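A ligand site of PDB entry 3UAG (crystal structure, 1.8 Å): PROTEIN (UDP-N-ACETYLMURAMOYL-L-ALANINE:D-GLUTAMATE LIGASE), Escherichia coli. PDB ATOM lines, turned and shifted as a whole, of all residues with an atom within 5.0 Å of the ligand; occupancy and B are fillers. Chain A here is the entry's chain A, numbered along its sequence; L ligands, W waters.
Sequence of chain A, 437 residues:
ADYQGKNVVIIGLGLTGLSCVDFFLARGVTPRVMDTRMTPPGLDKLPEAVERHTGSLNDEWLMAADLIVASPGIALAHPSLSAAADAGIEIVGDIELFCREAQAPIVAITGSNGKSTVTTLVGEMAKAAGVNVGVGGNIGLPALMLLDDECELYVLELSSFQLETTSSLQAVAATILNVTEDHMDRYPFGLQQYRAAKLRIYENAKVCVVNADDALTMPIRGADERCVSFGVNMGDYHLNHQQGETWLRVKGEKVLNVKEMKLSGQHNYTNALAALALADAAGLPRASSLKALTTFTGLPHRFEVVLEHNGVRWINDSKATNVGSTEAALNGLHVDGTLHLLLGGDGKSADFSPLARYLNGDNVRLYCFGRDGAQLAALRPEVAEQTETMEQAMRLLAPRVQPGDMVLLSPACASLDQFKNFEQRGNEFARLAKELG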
ATOM      1  N   GLY A 111     -15.732  22.748 -15.409  1.00  0.00           N
ATOM      2  CA  GLY A 111     -16.656  23.852 -15.199  1.00  0.00           C
ATOM      3  C   GLY A 111     -17.715  23.798 -16.288  1.00  0.00           C
ATOM      4  O   GLY A 111     -17.518  23.194 -17.349  1.00  0.00           O
ATOM      5  N   SER A 112     -18.841  24.478 -16.054  1.00  0.00           N
ATOM      6  CA  SER A 112     -19.925  24.469 -17.013  1.00  0.00           C
ATOM      7  C   SER A 112     -19.570  25.251 -18.280  1.00  0.00           C
ATOM      8  O   SER A 112     -19.943  24.831 -19.380  1.00  0.00           O
ATOM      9  CB  SER A 112     -21.189  25.019 -16.369  1.00  0.00           C
ATOM     10  OG  SER A 112     -21.571  24.195 -15.279  1.00  0.00           O
ATOM     11  N   ASN A 113     -18.772  26.312 -18.132  1.00  0.00           N
ATOM     12  CA  ASN A 113     -18.361  27.184 -19.241  1.00  0.00           C
ATOM     13  C   ASN A 113     -16.959  27.733 -19.022  1.00  0.00           C
ATOM     14  O   ASN A 113     -16.561  27.947 -17.878  1.00  0.00           O
ATOM     15  CB  ASN A 113     -19.328  28.354 -19.380  1.00  0.00           C
ATOM     16  CG  ASN A 113     -20.675  27.932 -19.910  1.00  0.00           C
ATOM     17  OD1 ASN A 113     -20.740  27.338 -21.001  1.00  0.00           O
ATOM     18  ND2 ASN A 113     -21.733  28.112 -19.109  1.00  0.00           N
ATOM     19  N   GLY A 114     -16.272  28.017 -20.120  1.00  0.00           N
ATOM     20  CA  GLY A 114     -14.953  28.620 -20.072  1.00  0.00           C
ATOM     21  C   GLY A 114     -13.816  27.641 -20.104  1.00  0.00           C
ATOM     22  O   GLY A 114     -12.664  28.041 -20.162  1.00  0.00           O
ATOM     23  N   LYS A 115     -14.114  26.333 -20.048  1.00  0.00           N
ATOM     24  CA  LYS A 115     -13.034  25.324 -19.945  1.00  0.00           C
ATOM     25  C   LYS A 115     -11.998  25.417 -21.115  1.00  0.00           C
ATOM     26  O   LYS A 115     -10.784  25.417 -20.870  1.00  0.00           O
ATOM     27  CB  LYS A 115     -13.577  23.884 -19.876  1.00  0.00           C
ATOM     28  CG  LYS A 115     -14.571  23.568 -18.771  1.00  0.00           C
ATOM     29  CD  LYS A 115     -15.006  22.058 -18.825  1.00  0.00           C
ATOM     30  CE  LYS A 115     -15.922  21.730 -19.991  1.00  0.00           C
ATOM     31  NZ  LYS A 115     -17.170  22.519 -19.913  1.00  0.00           N
ATOM     32  N   SER A 116     -12.458  25.481 -22.368  1.00  0.00           N
ATOM     33  CA  SER A 116     -11.512  25.469 -23.495  1.00  0.00           C
ATOM     34  C   SER A 116     -10.699  26.739 -23.478  1.00  0.00           C
ATOM     35  O   SER A 116      -9.511  26.730 -23.802  1.00  0.00           O
ATOM     36  CB  SER A 116     -12.221  25.374 -24.837  1.00  0.00           C
ATOM     37  OG  SER A 116     -12.965  24.183 -24.971  1.00  0.00           O
ATOM     38  N   THR A 117     -11.351  27.851 -23.155  1.00  0.00           N
ATOM     39  CA  THR A 117     -10.656  29.128 -23.074  1.00  0.00           C
ATOM     40  C   THR A 117      -9.538  29.089 -22.014  1.00  0.00           C
ATOM     41  O   THR A 117      -8.381  29.402 -22.323  1.00  0.00           O
ATOM     42  CB  THR A 117     -11.653  30.257 -22.782  1.00  0.00           C
ATOM     43  OG1 THR A 117     -12.582  30.323 -23.878  1.00  0.00           O
ATOM     44  CG2 THR A 117     -10.962  31.613 -22.685  1.00  0.00           C
ATOM     45  N   GLU A 157      -8.481  19.869 -20.503  1.00  0.00           N
ATOM     46  CA  GLU A 157      -9.909  20.184 -20.335  1.00  0.00           C
ATOM     47  C   GLU A 157     -10.681  18.903 -20.022  1.00  0.00           C
ATOM     48  O   GLU A 157     -10.639  17.946 -20.798  1.00  0.00           O
ATOM     49  CB  GLU A 157     -10.498  20.821 -21.597  1.00  0.00           C
ATOM     50  CG  GLU A 157     -12.030  21.019 -21.450  1.00  0.00           C
ATOM     51  CD  GLU A 157     -12.668  21.677 -22.646  1.00  0.00           C
ATOM     52  OE1 GLU A 157     -11.959  22.385 -23.381  1.00  0.00           O
ATOM     53  OE2 GLU A 157     -13.897  21.527 -22.834  1.00  0.00           O
ATOM     54  N   ASN A 178     -16.977  27.120 -12.771  1.00  0.00           N
ATOM     55  CA  ASN A 178     -18.345  27.512 -12.450  1.00  0.00           C
ATOM     56  C   ASN A 178     -19.239  26.290 -12.592  1.00  0.00           C
ATOM     57  O   ASN A 178     -18.862  25.317 -13.241  1.00  0.00           O
ATOM     58  CB  ASN A 178     -18.836  28.664 -13.370  1.00  0.00           C
ATOM     59  CG  ASN A 178     -18.566  28.398 -14.841  1.00  0.00           C
ATOM     60  OD1 ASN A 178     -19.155  27.515 -15.418  1.00  0.00           O
ATOM     61  ND2 ASN A 178     -17.625  29.107 -15.417  1.00  0.00           N
ATOM     62  N   HIS A 267     -16.359  37.726 -17.938  1.00  0.00           N
ATOM     63  CA  HIS A 267     -16.088  36.313 -17.739  1.00  0.00           C
ATOM     64  C   HIS A 267     -14.760  35.926 -18.344  1.00  0.00           C
ATOM     65  O   HIS A 267     -14.127  34.968 -17.887  1.00  0.00           O
ATOM     66  CB  HIS A 267     -17.217  35.459 -18.317  1.00  0.00           C
ATOM     67  CG  HIS A 267     -17.543  35.764 -19.746  1.00  0.00           C
ATOM     68  ND1 HIS A 267     -18.241  36.895 -20.094  1.00  0.00           N
ATOM     69  CD2 HIS A 267     -17.159  35.104 -20.869  1.00  0.00           C
ATOM     70  CE1 HIS A 267     -18.265  36.900 -21.418  1.00  0.00           C
ATOM     71  NE2 HIS A 267     -17.630  35.839 -21.926  1.00  0.00           N
ATOM     72  N   ASN A 268     -14.301  36.672 -19.365  1.00  0.00           N
ATOM     73  CA  ASN A 268     -12.996  36.372 -19.963  1.00  0.00           C
ATOM     74  C   ASN A 268     -11.869  36.944 -19.128  1.00  0.00           C
ATOM     75  O   ASN A 268     -10.794  36.351 -19.046  1.00  0.00           O
ATOM     76  CB  ASN A 268     -12.915  36.848 -21.407  1.00  0.00           C
ATOM     77  CG  ASN A 268     -13.573  35.872 -22.363  1.00  0.00           C
ATOM     78  OD1 ASN A 268     -13.492  34.650 -22.202  1.00  0.00           O
ATOM     79  ND2 ASN A 268     -14.251  36.400 -23.351  1.00  0.00           N
ATOM     80  N   THR A 270     -12.183  36.997 -15.737  1.00  0.00           N
ATOM     81  CA  THR A 270     -12.058  35.980 -14.687  1.00  0.00           C
ATOM     82  C   THR A 270     -11.498  34.652 -15.223  1.00  0.00           C
ATOM     83  O   THR A 270     -10.783  33.960 -14.496  1.00  0.00           O
ATOM     84  CB  THR A 270     -13.377  35.766 -13.888  1.00  0.00           C
ATOM     85  OG1 THR A 270     -14.430  35.351 -14.767  1.00  0.00           O
ATOM     86  CG2 THR A 270     -13.788  37.067 -13.173  1.00  0.00           C
ATOM     87  N   ASN A 271     -11.689  34.354 -16.511  1.00  0.00           N
ATOM     88  CA  ASN A 271     -11.010  33.198 -17.117  1.00  0.00           C
ATOM     89  C   ASN A 271      -9.494  33.410 -17.091  1.00  0.00           C
ATOM     90  O   ASN A 271      -8.726  32.473 -16.834  1.00  0.00           O
ATOM     91  CB  ASN A 271     -11.419  32.951 -18.568  1.00  0.00           C
ATOM     92  CG  ASN A 271     -12.807  32.331 -18.716  1.00  0.00           C
ATOM     93  OD1 ASN A 271     -13.401  31.801 -17.760  1.00  0.00           O
ATOM     94  ND2 ASN A 271     -13.366  32.432 -19.911  1.00  0.00           N
ATOM     95  N   LEU A 299     -10.853  31.561 -29.123  1.00  0.00           N
ATOM     96  CA  LEU A 299     -11.039  30.361 -29.900  1.00  0.00           C
ATOM     97  C   LEU A 299     -12.132  30.578 -30.937  1.00  0.00           C
ATOM     98  O   LEU A 299     -13.123  31.293 -30.679  1.00  0.00           O
ATOM     99  CB  LEU A 299     -11.395  29.205 -28.975  1.00  0.00           C
ATOM    100  CG  LEU A 299     -10.320  28.958 -27.931  1.00  0.00           C
ATOM    101  CD1 LEU A 299     -10.798  27.884 -26.968  1.00  0.00           C
ATOM    102  CD2 LEU A 299      -9.030  28.530 -28.620  1.00  0.00           C
ATOM    103  N   ARG A 302     -16.220  30.625 -30.177  1.00  0.00           N
ATOM    104  CA  ARG A 302     -16.516  31.210 -28.853  1.00  0.00           C
ATOM    105  C   ARG A 302     -16.685  32.705 -29.042  1.00  0.00           C
ATOM    106  O   ARG A 302     -15.680  33.415 -29.166  1.00  0.00           O
ATOM    107  CB  ARG A 302     -15.370  30.954 -27.843  1.00  0.00           C
ATOM    108  CG  ARG A 302     -15.276  29.537 -27.265  1.00  0.00           C
ATOM    109  CD  ARG A 302     -14.776  28.530 -28.306  1.00  0.00           C
ATOM    110  NE  ARG A 302     -14.526  27.224 -27.702  1.00  0.00           N
ATOM    111  CZ  ARG A 302     -14.018  26.175 -28.346  1.00  0.00           C
ATOM    112  NH1 ARG A 302     -13.700  26.280 -29.635  1.00  0.00           N
ATOM    113  NH2 ARG A 302     -13.762  25.050 -27.682  1.00  0.00           N
ATOM    114  N   PHE A 303     -17.932  33.171 -29.072  1.00  0.00           N
ATOM    115  CA  PHE A 303     -18.265  34.564 -29.444  1.00  0.00           C
ATOM    116  C   PHE A 303     -17.262  35.162 -30.467  1.00  0.00           C
ATOM    117  O   PHE A 303     -16.564  36.163 -30.205  1.00  0.00           O
ATOM    118  CB  PHE A 303     -18.352  35.439 -28.195  1.00  0.00           C
ATOM    119  CG  PHE A 303     -19.318  36.592 -28.327  1.00  0.00           C
ATOM    120  CD1 PHE A 303     -20.660  36.436 -27.967  1.00  0.00           C
ATOM    121  CD2 PHE A 303     -18.889  37.835 -28.795  1.00  0.00           C
ATOM    122  CE1 PHE A 303     -21.557  37.501 -28.085  1.00  0.00           C
ATOM    123  CE2 PHE A 303     -19.778  38.920 -28.917  1.00  0.00           C
ATOM    124  CZ  PHE A 303     -21.119  38.746 -28.551  1.00  0.00           C
ATOM    125  N   ASP A 317     -21.126  32.079 -31.999  1.00  0.00           N
ATOM    126  CA  ASP A 317     -20.957  31.630 -30.629  1.00  0.00           C
ATOM    127  C   ASP A 317     -21.532  30.218 -30.567  1.00  0.00           C
ATOM    128  O   ASP A 317     -22.208  29.853 -29.612  1.00  0.00           O
ATOM    129  CB  ASP A 317     -21.688  32.578 -29.673  1.00  0.00           C
ATOM    130  CG  ASP A 317     -21.248  32.436 -28.246  1.00  0.00           C
ATOM    131  OD1 ASP A 317     -20.099  31.973 -28.014  1.00  0.00           O
ATOM    132  OD2 ASP A 317     -22.028  32.845 -27.339  1.00  0.00           O
ATOM    133  N   LYS A 319     -20.277  27.578 -29.629  1.00  0.00           N
ATOM    134  CA  LYS A 319     -19.880  26.847 -28.429  1.00  0.00           C
ATOM    135  C   LYS A 319     -20.657  27.298 -27.188  1.00  0.00           C
ATOM    136  O   LYS A 319     -20.366  26.830 -26.072  1.00  0.00           O
ATOM    137  CB  LYS A 319     -18.390  27.004 -28.163  1.00  0.00           C
ATOM    138  CG  LYS A 319     -17.682  25.691 -28.034  1.00  0.00           C
ATOM    139  CD  LYS A 319     -18.292  24.788 -26.989  1.00  0.00           C
ATOM    140  CE  LYS A 319     -17.479  23.507 -26.843  1.00  0.00           C
ATOM    141  NZ  LYS A 319     -17.596  22.943 -25.466  1.00  0.00           N
ATOM    142  N   ALA A 320     -21.645  28.183 -27.356  1.00  0.00           N
ATOM    143  CA  ALA A 320     -22.582  28.456 -26.271  1.00  0.00           C
ATOM    144  C   ALA A 320     -23.627  27.340 -26.303  1.00  0.00           C
ATOM    145  O   ALA A 320     -24.582  27.378 -27.081  1.00  0.00           O
ATOM    146  CB  ALA A 320     -23.253  29.807 -26.447  1.00  0.00           C
ATOM    147  N   GLY A 324     -25.942  29.269 -19.374  1.00  0.00           N
ATOM    148  CA  GLY A 324     -24.927  30.147 -18.803  1.00  0.00           C
ATOM    149  C   GLY A 324     -24.111  30.847 -19.877  1.00  0.00           C
ATOM    150  O   GLY A 324     -23.800  32.023 -19.733  1.00  0.00           O
ATOM    151  N   SER A 325     -23.717  30.148 -20.930  1.00  0.00           N
ATOM    152  CA  SER A 325     -22.865  30.768 -21.935  1.00  0.00           C
ATOM    153  C   SER A 325     -23.652  31.773 -22.786  1.00  0.00           C
ATOM    154  O   SER A 325     -23.137  32.842 -23.129  1.00  0.00           O
ATOM    155  CB  SER A 325     -22.189  29.717 -22.816  1.00  0.00           C
ATOM    156  OG  SER A 325     -23.049  28.640 -23.095  1.00  0.00           O
ATOM    157  N   ALA A 328     -24.013  34.808 -20.748  1.00  0.00           N
ATOM    158  CA  ALA A 328     -22.779  35.568 -20.818  1.00  0.00           C
ATOM    159  C   ALA A 328     -22.629  36.377 -22.106  1.00  0.00           C
ATOM    160  O   ALA A 328     -22.072  37.483 -22.102  1.00  0.00           O
ATOM    161  CB  ALA A 328     -21.568  34.644 -20.610  1.00  0.00           C
HETATM  162  P1  LIG L   1     -16.408  25.089 -22.489  1.00  0.00           P
HETATM  163  O1  LIG L   1     -15.191  24.369 -23.154  1.00  0.00           O
HETATM  164  O2  LIG L   1     -16.586  24.842 -21.105  1.00  0.00           O
HETATM  165  O3  LIG L   1     -17.704  24.999 -23.195  1.00  0.00           O
HETATM  166  P2  LIG L   1     -15.439  27.566 -23.773  1.00  0.00           P
HETATM  167  O4  LIG L   1     -15.250  26.767 -24.966  1.00  0.00           O
HETATM  168  O5  LIG L   1     -14.220  28.336 -23.415  1.00  0.00           O
HETATM  169  O6  LIG L   1     -15.942  26.693 -22.536  1.00  0.00           O
HETATM  170  O7  LIG L   1     -16.659  28.542 -23.924  1.00  0.00           O
HETATM  171  C1  LIG L   1     -17.998  28.056 -24.454  1.00  0.00           C
HETATM  172  C2  LIG L   1     -19.043  29.160 -24.166  1.00  0.00           C
HETATM  173  O8  LIG L   1     -18.768  29.678 -22.864  1.00  0.00           O
HETATM  174  C3  LIG L   1     -18.811  30.232 -25.227  1.00  0.00           C
HETATM  175  O9  LIG L   1     -20.118  30.702 -25.634  1.00  0.00           O
HETATM  176  C4  LIG L   1     -18.169  31.420 -24.358  1.00  0.00           C
HETATM  177  O10 LIG L   1     -18.351  32.810 -24.666  1.00  0.00           O
HETATM  178  C5  LIG L   1     -18.736  31.129 -22.963  1.00  0.00           C
HETATM  179  N1  LIG L   1     -17.993  31.546 -21.764  1.00  0.00           N
HETATM  180  C6  LIG L   1     -16.636  31.541 -21.642  1.00  0.00           C
HETATM  181  N2  LIG L   1     -16.178  31.616 -20.414  1.00  0.00           N
HETATM  182  C7  LIG L   1     -17.333  31.695 -19.681  1.00  0.00           C
HETATM  183  C8  LIG L   1     -17.545  31.796 -18.237  1.00  0.00           C
HETATM  184  N3  LIG L   1     -16.499  31.808 -17.387  1.00  0.00           N
HETATM  185  N4  LIG L   1     -18.854  31.868 -17.869  1.00  0.00           N
HETATM  186  C9  LIG L   1     -19.885  31.841 -18.731  1.00  0.00           C
HETATM  187  N5  LIG L   1     -19.756  31.720 -20.071  1.00  0.00           N
HETATM  188  C10 LIG L   1     -18.462  31.658 -20.468  1.00  0.00           C
HETATM  189  O   HOH W   1     -19.372  35.857 -24.613  1.00  0.00           O
HETATM  190  O   HOH W   2     -14.053  32.593 -15.099  1.00  0.00           O
HETATM  191  O   HOH W   3     -19.635  32.768 -15.518  1.00  0.00           O
HETATM  192  O   HOH W   4     -14.432  32.662 -23.839  1.00  0.00           O
HETATM  193  O   HOH W   5     -19.848  24.179 -22.029  1.00  0.00           O
HETATM  194  O   HOH W   6     -16.326  34.702 -24.962  1.00  0.00           O
HETATM  195  O   HOH W   7     -16.116  31.348 -14.248  1.00  0.00           O
HETATM  196  O   HOH W   8     -21.006  33.534 -24.907  1.00  0.00           O
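Water W5 lies within hydrogen-bond range of an oxygen (O3) of the ligand (2.6 Å), the backbone carbonyl oxygen (O) of Ser 112 (2.7 Å) and the side-chain amide oxygen (OD1) of Asn 113 (3.4 Å).
Water W6 lies within hydrogen-bond range of an oxygen (O10) of the ligand (2.8 Å), the side-chain amide nitrogen of Asn 268 (3.1 Å) and a ring nitrogen (NE2) of His 267 (3.5 Å).
Water W7 lies within hydrogen-bond range of ND2 of Asn 178 and N3 of the ligand.
Water W1 lies within hydrogen-bond range of NE2 of His 267 (3.2 Å) and O10 of the ligand (3.2 Å).
Water W4 lies within hydrogen-bond range of the side-chain amide oxygen of Asn 268 (2.7 Å) and the side-chain hydroxyl of Thr 117 (3.0 Å).
Water W2 lies within hydrogen-bond range of the side-chain hydroxyl of Thr 270 (2.8 Å), the side-chain amide oxygen of Asn 271 (2.9 Å) and a nitrogen (N3) of the ligand (3.4 Å).
The side-chain carboxylate (OD1) of Asp 317 lies within hydrogen-bond range of the backbone NH (N) of Phe 303, at 2.7 Å.
The side-chain carboxylate of Glu 157 is in hydrogen-bond range of the side-chain hydroxyl of Ser 116, at 2.6 Å.
The side-chain amide oxygen (OD1) of Asn 271 lies close to the backbone carbonyl oxygen (O) of His 267 (3.3 Å).
The backbone NH (N) of Ser 325 lies close to the side-chain amide nitrogen (ND2) of Asn 113 (3.4 Å).
The backbone carbonyl oxygen (O) of Asn 178 is in hydrogen-bond range of the backbone NH (N) of Ser 112 (2.9 Å).
The backbone carbonyl oxygen (O) of Asn 113 sits at hydrogen-bond distance from the side-chain amide nitrogen (ND2) of Asn 178, at 2.9 Å.
O of His 267 lies within hydrogen-bond range of OG1 of Thr 270 (3.2 Å).
OD1 of Asn 268 lies within hydrogen-bond range of ND2 of Asn 271 (3.2 Å).
The side-chain hydroxyl of Ser 116 sits at hydrogen-bond distance from an oxygen (O1) of the ligand, 2.9 Å away.
An oxygen (O6) of the ligand is in hydrogen-bond range of the backbone NH (N) of Gly 114.
N of Ser 116 sits at hydrogen-bond distance from O1 of the ligand, 3.1 Å away.
NZ of Lys 319 lies within salt-bridge range of O3 of the ligand, 3.1 Å away.
An oxygen (O5) of the ligand is in hydrogen-bond range of the side-chain hydroxyl (OG1) of Thr 117 (2.6 Å).
An oxygen (O9) of the ligand sits close to the backbone NH (N) of Ala 320, 3.4 Å away.
The side-chain amide nitrogen (ND2) of Asn 271 lies within hydrogen-bond range of a nitrogen (N2) of the ligand (3.0 Å).
O5 of the ligand sits at hydrogen-bond distance from N of Thr 117 (2.9 Å).
The backbone NH (N) of Lys 115 is in hydrogen-bond range of an oxygen (O2) of the ligand (3.1 Å).
The side-chain carboxylate (OD1) of Asp 317 lies within hydrogen-bond range of an oxygen (O9) of the ligand (2.7 Å).
O2 of the ligand is in salt-bridge range of NZ of Lys 115 (2.7 Å).
The guanidinium group (NE) of Arg 302 is in salt-bridge range of an oxygen (O4) of the ligand (2.9 Å).
An oxygen (O1) of the ligand lies close to the side-chain carboxylate of Glu 157, 3.1 Å away.
Residues that only touch the ligand: Ser 325 (3.4 Å), Asn 113 (3.5 Å), Ala 328 (3.5 Å), Asn 178 (3.5 Å), His 267 (3.6 Å) and Ser 112 (3.8 Å).
Hydrophobic or aromatic side chains that line the ligand: His 267, Ala 320 and Ala 328.
Within 4 Å of the ligand: Ser 112, Asn 113, Gly 114, Lys 115, Ser 116, Thr 117, Glu 157, Asn 178, His 267, Asn 271, Arg 302, Asp 317, Lys 319, Ala 320, Ser 325 and Ala 328.
The nearest printed residue that does not touch the ligand is Gly 324 (4.05 Å).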
